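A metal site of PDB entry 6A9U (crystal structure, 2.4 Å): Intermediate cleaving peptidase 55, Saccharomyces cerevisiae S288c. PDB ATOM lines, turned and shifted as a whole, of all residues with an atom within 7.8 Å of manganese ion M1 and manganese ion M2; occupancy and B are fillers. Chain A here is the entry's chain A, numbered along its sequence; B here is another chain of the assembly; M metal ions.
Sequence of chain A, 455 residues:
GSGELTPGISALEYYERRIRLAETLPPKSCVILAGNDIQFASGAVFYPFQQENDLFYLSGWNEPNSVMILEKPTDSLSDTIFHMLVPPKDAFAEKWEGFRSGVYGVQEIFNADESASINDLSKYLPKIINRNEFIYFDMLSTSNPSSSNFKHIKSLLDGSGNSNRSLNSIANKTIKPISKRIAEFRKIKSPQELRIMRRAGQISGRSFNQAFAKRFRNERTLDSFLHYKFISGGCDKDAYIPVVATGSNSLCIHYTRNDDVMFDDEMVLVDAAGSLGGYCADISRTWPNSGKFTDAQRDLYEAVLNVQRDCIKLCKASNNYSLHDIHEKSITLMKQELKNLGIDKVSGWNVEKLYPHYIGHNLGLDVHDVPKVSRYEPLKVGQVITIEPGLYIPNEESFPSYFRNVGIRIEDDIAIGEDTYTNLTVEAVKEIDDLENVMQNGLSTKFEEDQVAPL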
ATOM      1  N   TYR A 240     -24.114  10.337  28.652  1.00  0.00           N
ATOM      2  CA  TYR A 240     -25.176  10.538  27.664  1.00  0.00           C
ATOM      3  C   TYR A 240     -26.425   9.831  28.174  1.00  0.00           C
ATOM      4  O   TYR A 240     -26.379   9.062  29.136  1.00  0.00           O
ATOM      5  CB  TYR A 240     -24.771  10.006  26.279  1.00  0.00           C
ATOM      6  CG  TYR A 240     -24.172   8.616  26.306  1.00  0.00           C
ATOM      7  CD1 TYR A 240     -24.976   7.479  26.206  1.00  0.00           C
ATOM      8  CD2 TYR A 240     -22.791   8.430  26.411  1.00  0.00           C
ATOM      9  CE1 TYR A 240     -24.427   6.200  26.235  1.00  0.00           C
ATOM     10  CE2 TYR A 240     -22.239   7.147  26.433  1.00  0.00           C
ATOM     11  CZ  TYR A 240     -23.061   6.038  26.346  1.00  0.00           C
ATOM     12  OH  TYR A 240     -22.519   4.775  26.365  1.00  0.00           O
ATOM     13  N   VAL A 243     -29.588   3.650  26.893  1.00  0.00           N
ATOM     14  CA  VAL A 243     -30.496   2.735  26.190  1.00  0.00           C
ATOM     15  C   VAL A 243     -30.595   1.436  26.982  1.00  0.00           C
ATOM     16  O   VAL A 243     -29.575   0.806  27.277  1.00  0.00           O
ATOM     17  CB  VAL A 243     -30.020   2.455  24.758  1.00  0.00           C
ATOM     18  CG1 VAL A 243     -30.955   1.465  24.062  1.00  0.00           C
ATOM     19  CG2 VAL A 243     -29.911   3.741  23.942  1.00  0.00           C
ATOM     20  N   VAL A 270     -27.852  -2.889  26.072  1.00  0.00           N
ATOM     21  CA  VAL A 270     -27.619  -1.752  26.966  1.00  0.00           C
ATOM     22  C   VAL A 270     -26.452  -0.916  26.448  1.00  0.00           C
ATOM     23  O   VAL A 270     -25.398  -1.462  26.117  1.00  0.00           O
ATOM     24  CB  VAL A 270     -27.364  -2.207  28.414  1.00  0.00           C
ATOM     25  CG1 VAL A 270     -26.956  -1.029  29.286  1.00  0.00           C
ATOM     26  CG2 VAL A 270     -28.598  -2.895  28.993  1.00  0.00           C
ATOM     27  N   ASP A 271     -26.635   0.407  26.424  1.00  0.00           N
ATOM     28  CA  ASP A 271     -25.597   1.370  26.014  1.00  0.00           C
ATOM     29  C   ASP A 271     -25.549   2.503  27.040  1.00  0.00           C
ATOM     30  O   ASP A 271     -26.462   3.328  27.082  1.00  0.00           O
ATOM     31  CB  ASP A 271     -25.907   1.915  24.616  1.00  0.00           C
ATOM     32  CG  ASP A 271     -24.701   2.601  23.978  1.00  0.00           C
ATOM     33  OD1 ASP A 271     -23.754   2.966  24.706  1.00  0.00           O
ATOM     34  OD2 ASP A 271     -24.707   2.796  22.740  1.00  0.00           O
ATOM     35  N   ALA A 272     -24.485   2.563  27.838  1.00  0.00           N
ATOM     36  CA  ALA A 272     -24.367   3.561  28.906  1.00  0.00           C
ATOM     37  C   ALA A 272     -22.936   3.594  29.434  1.00  0.00           C
ATOM     38  O   ALA A 272     -22.195   2.618  29.318  1.00  0.00           O
ATOM     39  CB  ALA A 272     -25.346   3.254  30.050  1.00  0.00           C
ATOM     40  N   ALA A 273     -22.568   4.731  30.045  1.00  0.00           N
ATOM     41  CA  ALA A 273     -21.238   4.959  30.595  1.00  0.00           C
ATOM     42  C   ALA A 273     -21.221   6.280  31.372  1.00  0.00           C
ATOM     43  O   ALA A 273     -22.161   7.076  31.285  1.00  0.00           O
ATOM     44  CB  ALA A 273     -20.165   4.985  29.498  1.00  0.00           C
ATOM     45  N   ALA A 281     -16.671   8.372  28.466  1.00  0.00           N
ATOM     46  CA  ALA A 281     -16.525   6.974  28.054  1.00  0.00           C
ATOM     47  C   ALA A 281     -17.787   6.542  27.293  1.00  0.00           C
ATOM     48  O   ALA A 281     -18.743   7.313  27.165  1.00  0.00           O
ATOM     49  CB  ALA A 281     -16.270   6.072  29.261  1.00  0.00           C
ATOM     50  N   ASP A 282     -17.784   5.297  26.786  1.00  0.00           N
ATOM     51  CA  ASP A 282     -18.857   4.817  25.911  1.00  0.00           C
ATOM     52  C   ASP A 282     -18.803   3.299  25.684  1.00  0.00           C
ATOM     53  O   ASP A 282     -17.838   2.803  25.083  1.00  0.00           O
ATOM     54  CB  ASP A 282     -18.778   5.560  24.566  1.00  0.00           C
ATOM     55  CG  ASP A 282     -20.018   5.396  23.704  1.00  0.00           C
ATOM     56  OD1 ASP A 282     -20.956   4.671  24.099  1.00  0.00           O
ATOM     57  OD2 ASP A 282     -20.054   6.008  22.614  1.00  0.00           O
ATOM     58  N   ILE A 283     -19.840   2.560  26.106  1.00  0.00           N
ATOM     59  CA  ILE A 283     -19.804   1.098  26.181  1.00  0.00           C
ATOM     60  C   ILE A 283     -21.149   0.504  25.741  1.00  0.00           C
ATOM     61  O   ILE A 283     -22.208   1.072  25.997  1.00  0.00           O
ATOM     62  CB  ILE A 283     -19.448   0.629  27.617  1.00  0.00           C
ATOM     63  CG1 ILE A 283     -17.979   0.961  27.950  1.00  0.00           C
ATOM     64  CG2 ILE A 283     -19.695  -0.865  27.811  1.00  0.00           C
ATOM     65  CD1 ILE A 283     -17.549   0.513  29.332  1.00  0.00           C
ATOM     66  N   SER A 284     -21.088  -0.670  25.074  1.00  0.00           N
ATOM     67  CA  SER A 284     -22.261  -1.460  24.691  1.00  0.00           C
ATOM     68  C   SER A 284     -22.037  -2.946  24.954  1.00  0.00           C
ATOM     69  O   SER A 284     -20.955  -3.466  24.657  1.00  0.00           O
ATOM     70  CB  SER A 284     -22.608  -1.266  23.203  1.00  0.00           C
ATOM     71  OG  SER A 284     -23.093   0.033  22.909  1.00  0.00           O
ATOM     72  N   ILE A 359     -19.235   2.697  11.625  1.00  0.00           N
ATOM     73  CA  ILE A 359     -18.419   1.811  12.461  1.00  0.00           C
ATOM     74  C   ILE A 359     -17.944   2.474  13.764  1.00  0.00           C
ATOM     75  O   ILE A 359     -17.697   1.775  14.747  1.00  0.00           O
ATOM     76  CB  ILE A 359     -17.227   1.281  11.633  1.00  0.00           C
ATOM     77  CG1 ILE A 359     -16.444   0.200  12.405  1.00  0.00           C
ATOM     78  CG2 ILE A 359     -16.283   2.410  11.238  1.00  0.00           C
ATOM     79  CD1 ILE A 359     -17.128  -1.145  12.468  1.00  0.00           C
ATOM     80  N   GLY A 360     -17.829   3.805  13.812  1.00  0.00           N
ATOM     81  CA  GLY A 360     -17.337   4.458  15.018  1.00  0.00           C
ATOM     82  C   GLY A 360     -17.148   5.946  14.853  1.00  0.00           C
ATOM     83  O   GLY A 360     -17.650   6.541  13.894  1.00  0.00           O
ATOM     84  N   HIS A 361     -16.418   6.554  15.794  1.00  0.00           N
ATOM     85  CA  HIS A 361     -16.233   8.006  15.853  1.00  0.00           C
ATOM     86  C   HIS A 361     -15.105   8.347  16.827  1.00  0.00           C
ATOM     87  O   HIS A 361     -14.690   7.525  17.644  1.00  0.00           O
ATOM     88  CB  HIS A 361     -17.538   8.699  16.254  1.00  0.00           C
ATOM     89  CG  HIS A 361     -18.132   8.169  17.534  1.00  0.00           C
ATOM     90  ND1 HIS A 361     -17.840   8.698  18.774  1.00  0.00           N
ATOM     91  CD2 HIS A 361     -18.990   7.148  17.749  1.00  0.00           C
ATOM     92  CE1 HIS A 361     -18.495   8.020  19.698  1.00  0.00           C
ATOM     93  NE2 HIS A 361     -19.205   7.080  19.104  1.00  0.00           N
ATOM     94  N   ASN A 362     -14.632   9.600  16.738  1.00  0.00           N
ATOM     95  CA  ASN A 362     -13.665  10.153  17.688  1.00  0.00           C
ATOM     96  C   ASN A 362     -14.326  10.409  19.044  1.00  0.00           C
ATOM     97  O   ASN A 362     -15.536  10.641  19.142  1.00  0.00           O
ATOM     98  CB  ASN A 362     -13.073  11.466  17.155  1.00  0.00           C
ATOM     99  CG  ASN A 362     -11.835  11.255  16.280  1.00  0.00           C
ATOM    100  OD1 ASN A 362     -10.726  11.064  16.785  1.00  0.00           O
ATOM    101  ND2 ASN A 362     -12.016  11.325  14.966  1.00  0.00           N
ATOM    102  N   LEU A 363     -13.503  10.393  20.111  1.00  0.00           N
ATOM    103  CA  LEU A 363     -13.995  10.487  21.481  1.00  0.00           C
ATOM    104  C   LEU A 363     -13.089  11.376  22.330  1.00  0.00           C
ATOM    105  O   LEU A 363     -11.863  11.252  22.277  1.00  0.00           O
ATOM    106  CB  LEU A 363     -14.082   9.091  22.136  1.00  0.00           C
ATOM    107  CG  LEU A 363     -14.647   8.998  23.553  1.00  0.00           C
ATOM    108  CD1 LEU A 363     -16.138   9.311  23.599  1.00  0.00           C
ATOM    109  CD2 LEU A 363     -14.374   7.625  24.152  1.00  0.00           C
ATOM    110  N   VAL A 367     -18.988  13.569  23.215  1.00  0.00           N
ATOM    111  CA  VAL A 367     -19.165  12.165  22.842  1.00  0.00           C
ATOM    112  C   VAL A 367     -18.819  11.959  21.376  1.00  0.00           C
ATOM    113  O   VAL A 367     -18.045  11.053  21.028  1.00  0.00           O
ATOM    114  CB  VAL A 367     -20.591  11.688  23.165  1.00  0.00           C
ATOM    115  CG1 VAL A 367     -20.758  10.227  22.779  1.00  0.00           C
ATOM    116  CG2 VAL A 367     -20.897  11.882  24.642  1.00  0.00           C
ATOM    117  N   HIS A 368     -19.369  12.791  20.497  1.00  0.00           N
ATOM    118  CA  HIS A 368     -18.961  12.832  19.092  1.00  0.00           C
ATOM    119  C   HIS A 368     -17.943  13.962  18.957  1.00  0.00           C
ATOM    120  O   HIS A 368     -18.250  15.086  18.566  1.00  0.00           O
ATOM    121  CB  HIS A 368     -20.164  13.024  18.183  1.00  0.00           C
ATOM    122  CG  HIS A 368     -21.067  11.832  18.108  1.00  0.00           C
ATOM    123  ND1 HIS A 368     -22.347  11.896  17.613  1.00  0.00           N
ATOM    124  CD2 HIS A 368     -20.861  10.543  18.486  1.00  0.00           C
ATOM    125  CE1 HIS A 368     -22.902  10.692  17.677  1.00  0.00           C
ATOM    126  NE2 HIS A 368     -22.026   9.861  18.205  1.00  0.00           N
ATOM    127  N   THR A 386     -13.880   4.680  18.628  1.00  0.00           N
ATOM    128  CA  THR A 386     -14.725   3.564  18.996  1.00  0.00           C
ATOM    129  C   THR A 386     -14.883   2.572  17.835  1.00  0.00           C
ATOM    130  O   THR A 386     -14.652   2.906  16.668  1.00  0.00           O
ATOM    131  CB  THR A 386     -16.119   4.036  19.444  1.00  0.00           C
ATOM    132  OG1 THR A 386     -16.795   4.661  18.348  1.00  0.00           O
ATOM    133  CG2 THR A 386     -16.007   5.029  20.598  1.00  0.00           C
ATOM    134  N   ILE A 387     -15.296   1.348  18.176  1.00  0.00           N
ATOM    135  CA  ILE A 387     -15.519   0.244  17.231  1.00  0.00           C
ATOM    136  C   ILE A 387     -16.788  -0.478  17.680  1.00  0.00           C
ATOM    137  O   ILE A 387     -16.783  -1.149  18.729  1.00  0.00           O
ATOM    138  CB  ILE A 387     -14.328  -0.728  17.190  1.00  0.00           C
ATOM    139  CG1 ILE A 387     -13.004   0.001  16.929  1.00  0.00           C
ATOM    140  CG2 ILE A 387     -14.563  -1.839  16.171  1.00  0.00           C
ATOM    141  CD1 ILE A 387     -12.734   0.364  15.471  1.00  0.00           C
ATOM    142  N   GLU A 388     -17.882  -0.382  16.894  1.00  0.00           N
ATOM    143  CA  GLU A 388     -19.206  -0.821  17.348  1.00  0.00           C
ATOM    144  C   GLU A 388     -20.094  -1.289  16.192  1.00  0.00           C
ATOM    145  O   GLU A 388     -21.093  -0.646  15.849  1.00  0.00           O
ATOM    146  CB  GLU A 388     -19.897   0.306  18.119  1.00  0.00           C
ATOM    147  CG  GLU A 388     -19.853   1.684  17.432  1.00  0.00           C
ATOM    148  CD  GLU A 388     -20.653   2.746  18.168  1.00  0.00           C
ATOM    149  OE1 GLU A 388     -20.193   3.910  18.219  1.00  0.00           O
ATOM    150  OE2 GLU A 388     -21.739   2.419  18.708  1.00  0.00           O
ATOM    151  N   ARG A 409     -25.275  -5.552  19.634  1.00  0.00           N
ATOM    152  CA  ARG A 409     -24.191  -4.601  19.394  1.00  0.00           C
ATOM    153  C   ARG A 409     -23.144  -4.720  20.502  1.00  0.00           C
ATOM    154  O   ARG A 409     -23.491  -4.948  21.671  1.00  0.00           O
ATOM    155  CB  ARG A 409     -24.722  -3.161  19.320  1.00  0.00           C
ATOM    156  CG  ARG A 409     -23.661  -2.106  18.966  1.00  0.00           C
ATOM    157  CD  ARG A 409     -24.266  -0.797  18.458  1.00  0.00           C
ATOM    158  NE  ARG A 409     -24.730   0.068  19.540  1.00  0.00           N
ATOM    159  CZ  ARG A 409     -25.987   0.477  19.691  1.00  0.00           C
ATOM    160  NH1 ARG A 409     -26.923   0.098  18.830  1.00  0.00           N
ATOM    161  NH2 ARG A 409     -26.308   1.266  20.703  1.00  0.00           N
ATOM    162  N   GLU A 411     -19.275  -2.832  21.769  1.00  0.00           N
ATOM    163  CA  GLU A 411     -18.501  -1.599  21.550  1.00  0.00           C
ATOM    164  C   GLU A 411     -17.437  -1.410  22.629  1.00  0.00           C
ATOM    165  O   GLU A 411     -17.676  -1.708  23.797  1.00  0.00           O
ATOM    166  CB  GLU A 411     -19.450  -0.382  21.496  1.00  0.00           C
ATOM    167  CG  GLU A 411     -18.868   0.990  21.909  1.00  0.00           C
ATOM    168  CD  GLU A 411     -19.853   2.138  21.697  1.00  0.00           C
ATOM    169  OE1 GLU A 411     -19.471   3.194  21.132  1.00  0.00           O
ATOM    170  OE2 GLU A 411     -21.035   1.975  22.071  1.00  0.00           O
ATOM    171  N   ASP A 412     -16.254  -0.914  22.218  1.00  0.00           N
ATOM    172  CA  ASP A 412     -15.128  -0.613  23.104  1.00  0.00           C
ATOM    173  C   ASP A 412     -14.402   0.657  22.626  1.00  0.00           C
ATOM    174  O   ASP A 412     -14.613   1.131  21.515  1.00  0.00           O
ATOM    175  CB  ASP A 412     -14.128  -1.779  23.175  1.00  0.00           C
ATOM    176  CG  ASP A 412     -14.656  -2.971  23.972  1.00  0.00           C
ATOM    177  OD1 ASP A 412     -15.304  -3.854  23.361  1.00  0.00           O
ATOM    178  OD2 ASP A 412     -14.404  -3.046  25.198  1.00  0.00           O
ATOM    179  N   ASP A 413     -13.518   1.192  23.478  1.00  0.00           N
ATOM    180  CA  ASP A 413     -12.759   2.405  23.190  1.00  0.00           C
ATOM    181  C   ASP A 413     -11.271   2.093  23.057  1.00  0.00           C
ATOM    182  O   ASP A 413     -10.679   1.472  23.959  1.00  0.00           O
ATOM    183  CB  ASP A 413     -12.971   3.452  24.300  1.00  0.00           C
ATOM    184  CG  ASP A 413     -14.438   3.663  24.643  1.00  0.00           C
ATOM    185  OD1 ASP A 413     -15.306   3.497  23.754  1.00  0.00           O
ATOM    186  OD2 ASP A 413     -14.739   4.013  25.806  1.00  0.00           O
ATOM    187  CB  01B B   1     -23.210   6.410  21.458  1.00  0.00           C
ATOM    188  CA  01B B   1     -23.254   5.347  20.346  1.00  0.00           C
ATOM    189  N   01B B   1     -23.641   5.841  22.707  1.00  0.00           N
ATOM    190  O2  01B B   1     -22.101   4.548  20.401  1.00  0.00           O
ATOM    191  C   01B B   1     -23.332   6.010  18.957  1.00  0.00           C
ATOM    192  C6  01B B   1     -24.110   7.639  21.103  1.00  0.00           C
ATOM    193  C7  01B B   1     -25.653   7.295  21.195  1.00  0.00           C
ATOM    194  C8  01B B   1     -26.353   6.896  20.067  1.00  0.00           C
ATOM    195  C9  01B B   1     -27.716   6.601  20.147  1.00  0.00           C
ATOM    196  C10 01B B   1     -28.383   6.710  21.363  1.00  0.00           C
ATOM    197  C11 01B B   1     -27.685   7.130  22.503  1.00  0.00           C
ATOM    198  C12 01B B   1     -26.327   7.415  22.414  1.00  0.00           C
ATOM    199  O   01B B   1     -22.386   6.727  18.545  1.00  0.00           O
ATOM    200  N   PRO B   2     -23.758   5.454  17.712  1.00  0.00           N
ATOM    201  CA  PRO B   2     -23.461   5.455  16.270  1.00  0.00           C
ATOM    202  C   PRO B   2     -23.725   6.820  15.619  1.00  0.00           C
ATOM    203  O   PRO B   2     -24.789   7.388  15.825  1.00  0.00           O
ATOM    204  CB  PRO B   2     -24.407   4.394  15.717  1.00  0.00           C
ATOM    205  CG  PRO B   2     -24.703   3.499  16.872  1.00  0.00           C
ATOM    206  CD  PRO B   2     -24.713   4.392  18.078  1.00  0.00           C
ATOM    207  N   PRO B   3     -22.762   7.311  14.841  1.00  0.00           N
ATOM    208  CA  PRO B   3     -22.923   8.633  14.209  1.00  0.00           C
ATOM    209  C   PRO B   3     -24.050   8.670  13.186  1.00  0.00           C
ATOM    210  O   PRO B   3     -25.016   9.422  13.343  1.00  0.00           O
ATOM    211  CB  PRO B   3     -21.555   8.868  13.545  1.00  0.00           C
ATOM    212  CG  PRO B   3     -20.617   7.968  14.282  1.00  0.00           C
ATOM    213  CD  PRO B   3     -21.423   6.750  14.612  1.00  0.00           C
HETATM  214 MN    MN M   1     -20.287   5.422  20.399  1.00  0.00          MN
HETATM  215 MN    MN M   2     -22.512   3.986  22.686  1.00  0.00          MN
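The backbone carbonyl oxygen of His 361 lies within hydrogen-bond range of the backbone NH of Thr 386 (3.1 Å).
The backbone carbonyl oxygen (O) of Ser 284 sits at hydrogen-bond distance from the backbone NH (N) of Glu 411 (3.4 Å).
The side-chain carboxylate of Asp 271 sits close to the side-chain hydroxyl of Ser 284, at 3.2 Å.
The guanidinium group (NH2) of Arg 409 lies close to the side-chain carboxylate (OD2) of Asp 271, at 3.0 Å.
N of Asp 271 lies within hydrogen-bond range of O of Val 243, 3.1 Å away.
OE1 of Glu 388 lies close to OG1 of Thr 386 (3.5 Å).
The backbone NH (N) of Ile 283 is in hydrogen-bond range of the side-chain hydroxyl (OH) of Tyr 240 (3.5 Å).
N of Ala 272 is in hydrogen-bond range of OH of Tyr 240.
Of the 27 residues printed, 5 come within 4 Å of manganese ion M1.
The nearest printed residue that does not touch manganese ion M1 is Thr 386 (4.1 Å).
Merely in contact with manganese ion M2: Tyr 240 (3.8 Å).
O2 of 01B 1 of chain B binds manganese ion M1.
Manganese ion M1 is bound by OD2 of Asp 282, 2.3 Å away.
Manganese ion M1 is bound by a ring nitrogen (NE2) of His 361, 2.4 Å away.
OE1 of Glu 411 binds manganese ion M1 (2.5 Å).
Manganese ion M1 is bound by OE1 of Glu 388.
Manganese ion M1 has five donor atoms within binding distance.
Manganese ion M2 is bound by N of 01B 1 of chain B (2.2 Å), OD1 of Asp 282 (2.2 Å), O2 of 01B 1 of chain B (2.4 Å), OD2 of Asp 271 (2.5 Å), OE2 of Glu 411 (2.6 Å) and OD1 of Asp 271 (2.6 Å).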
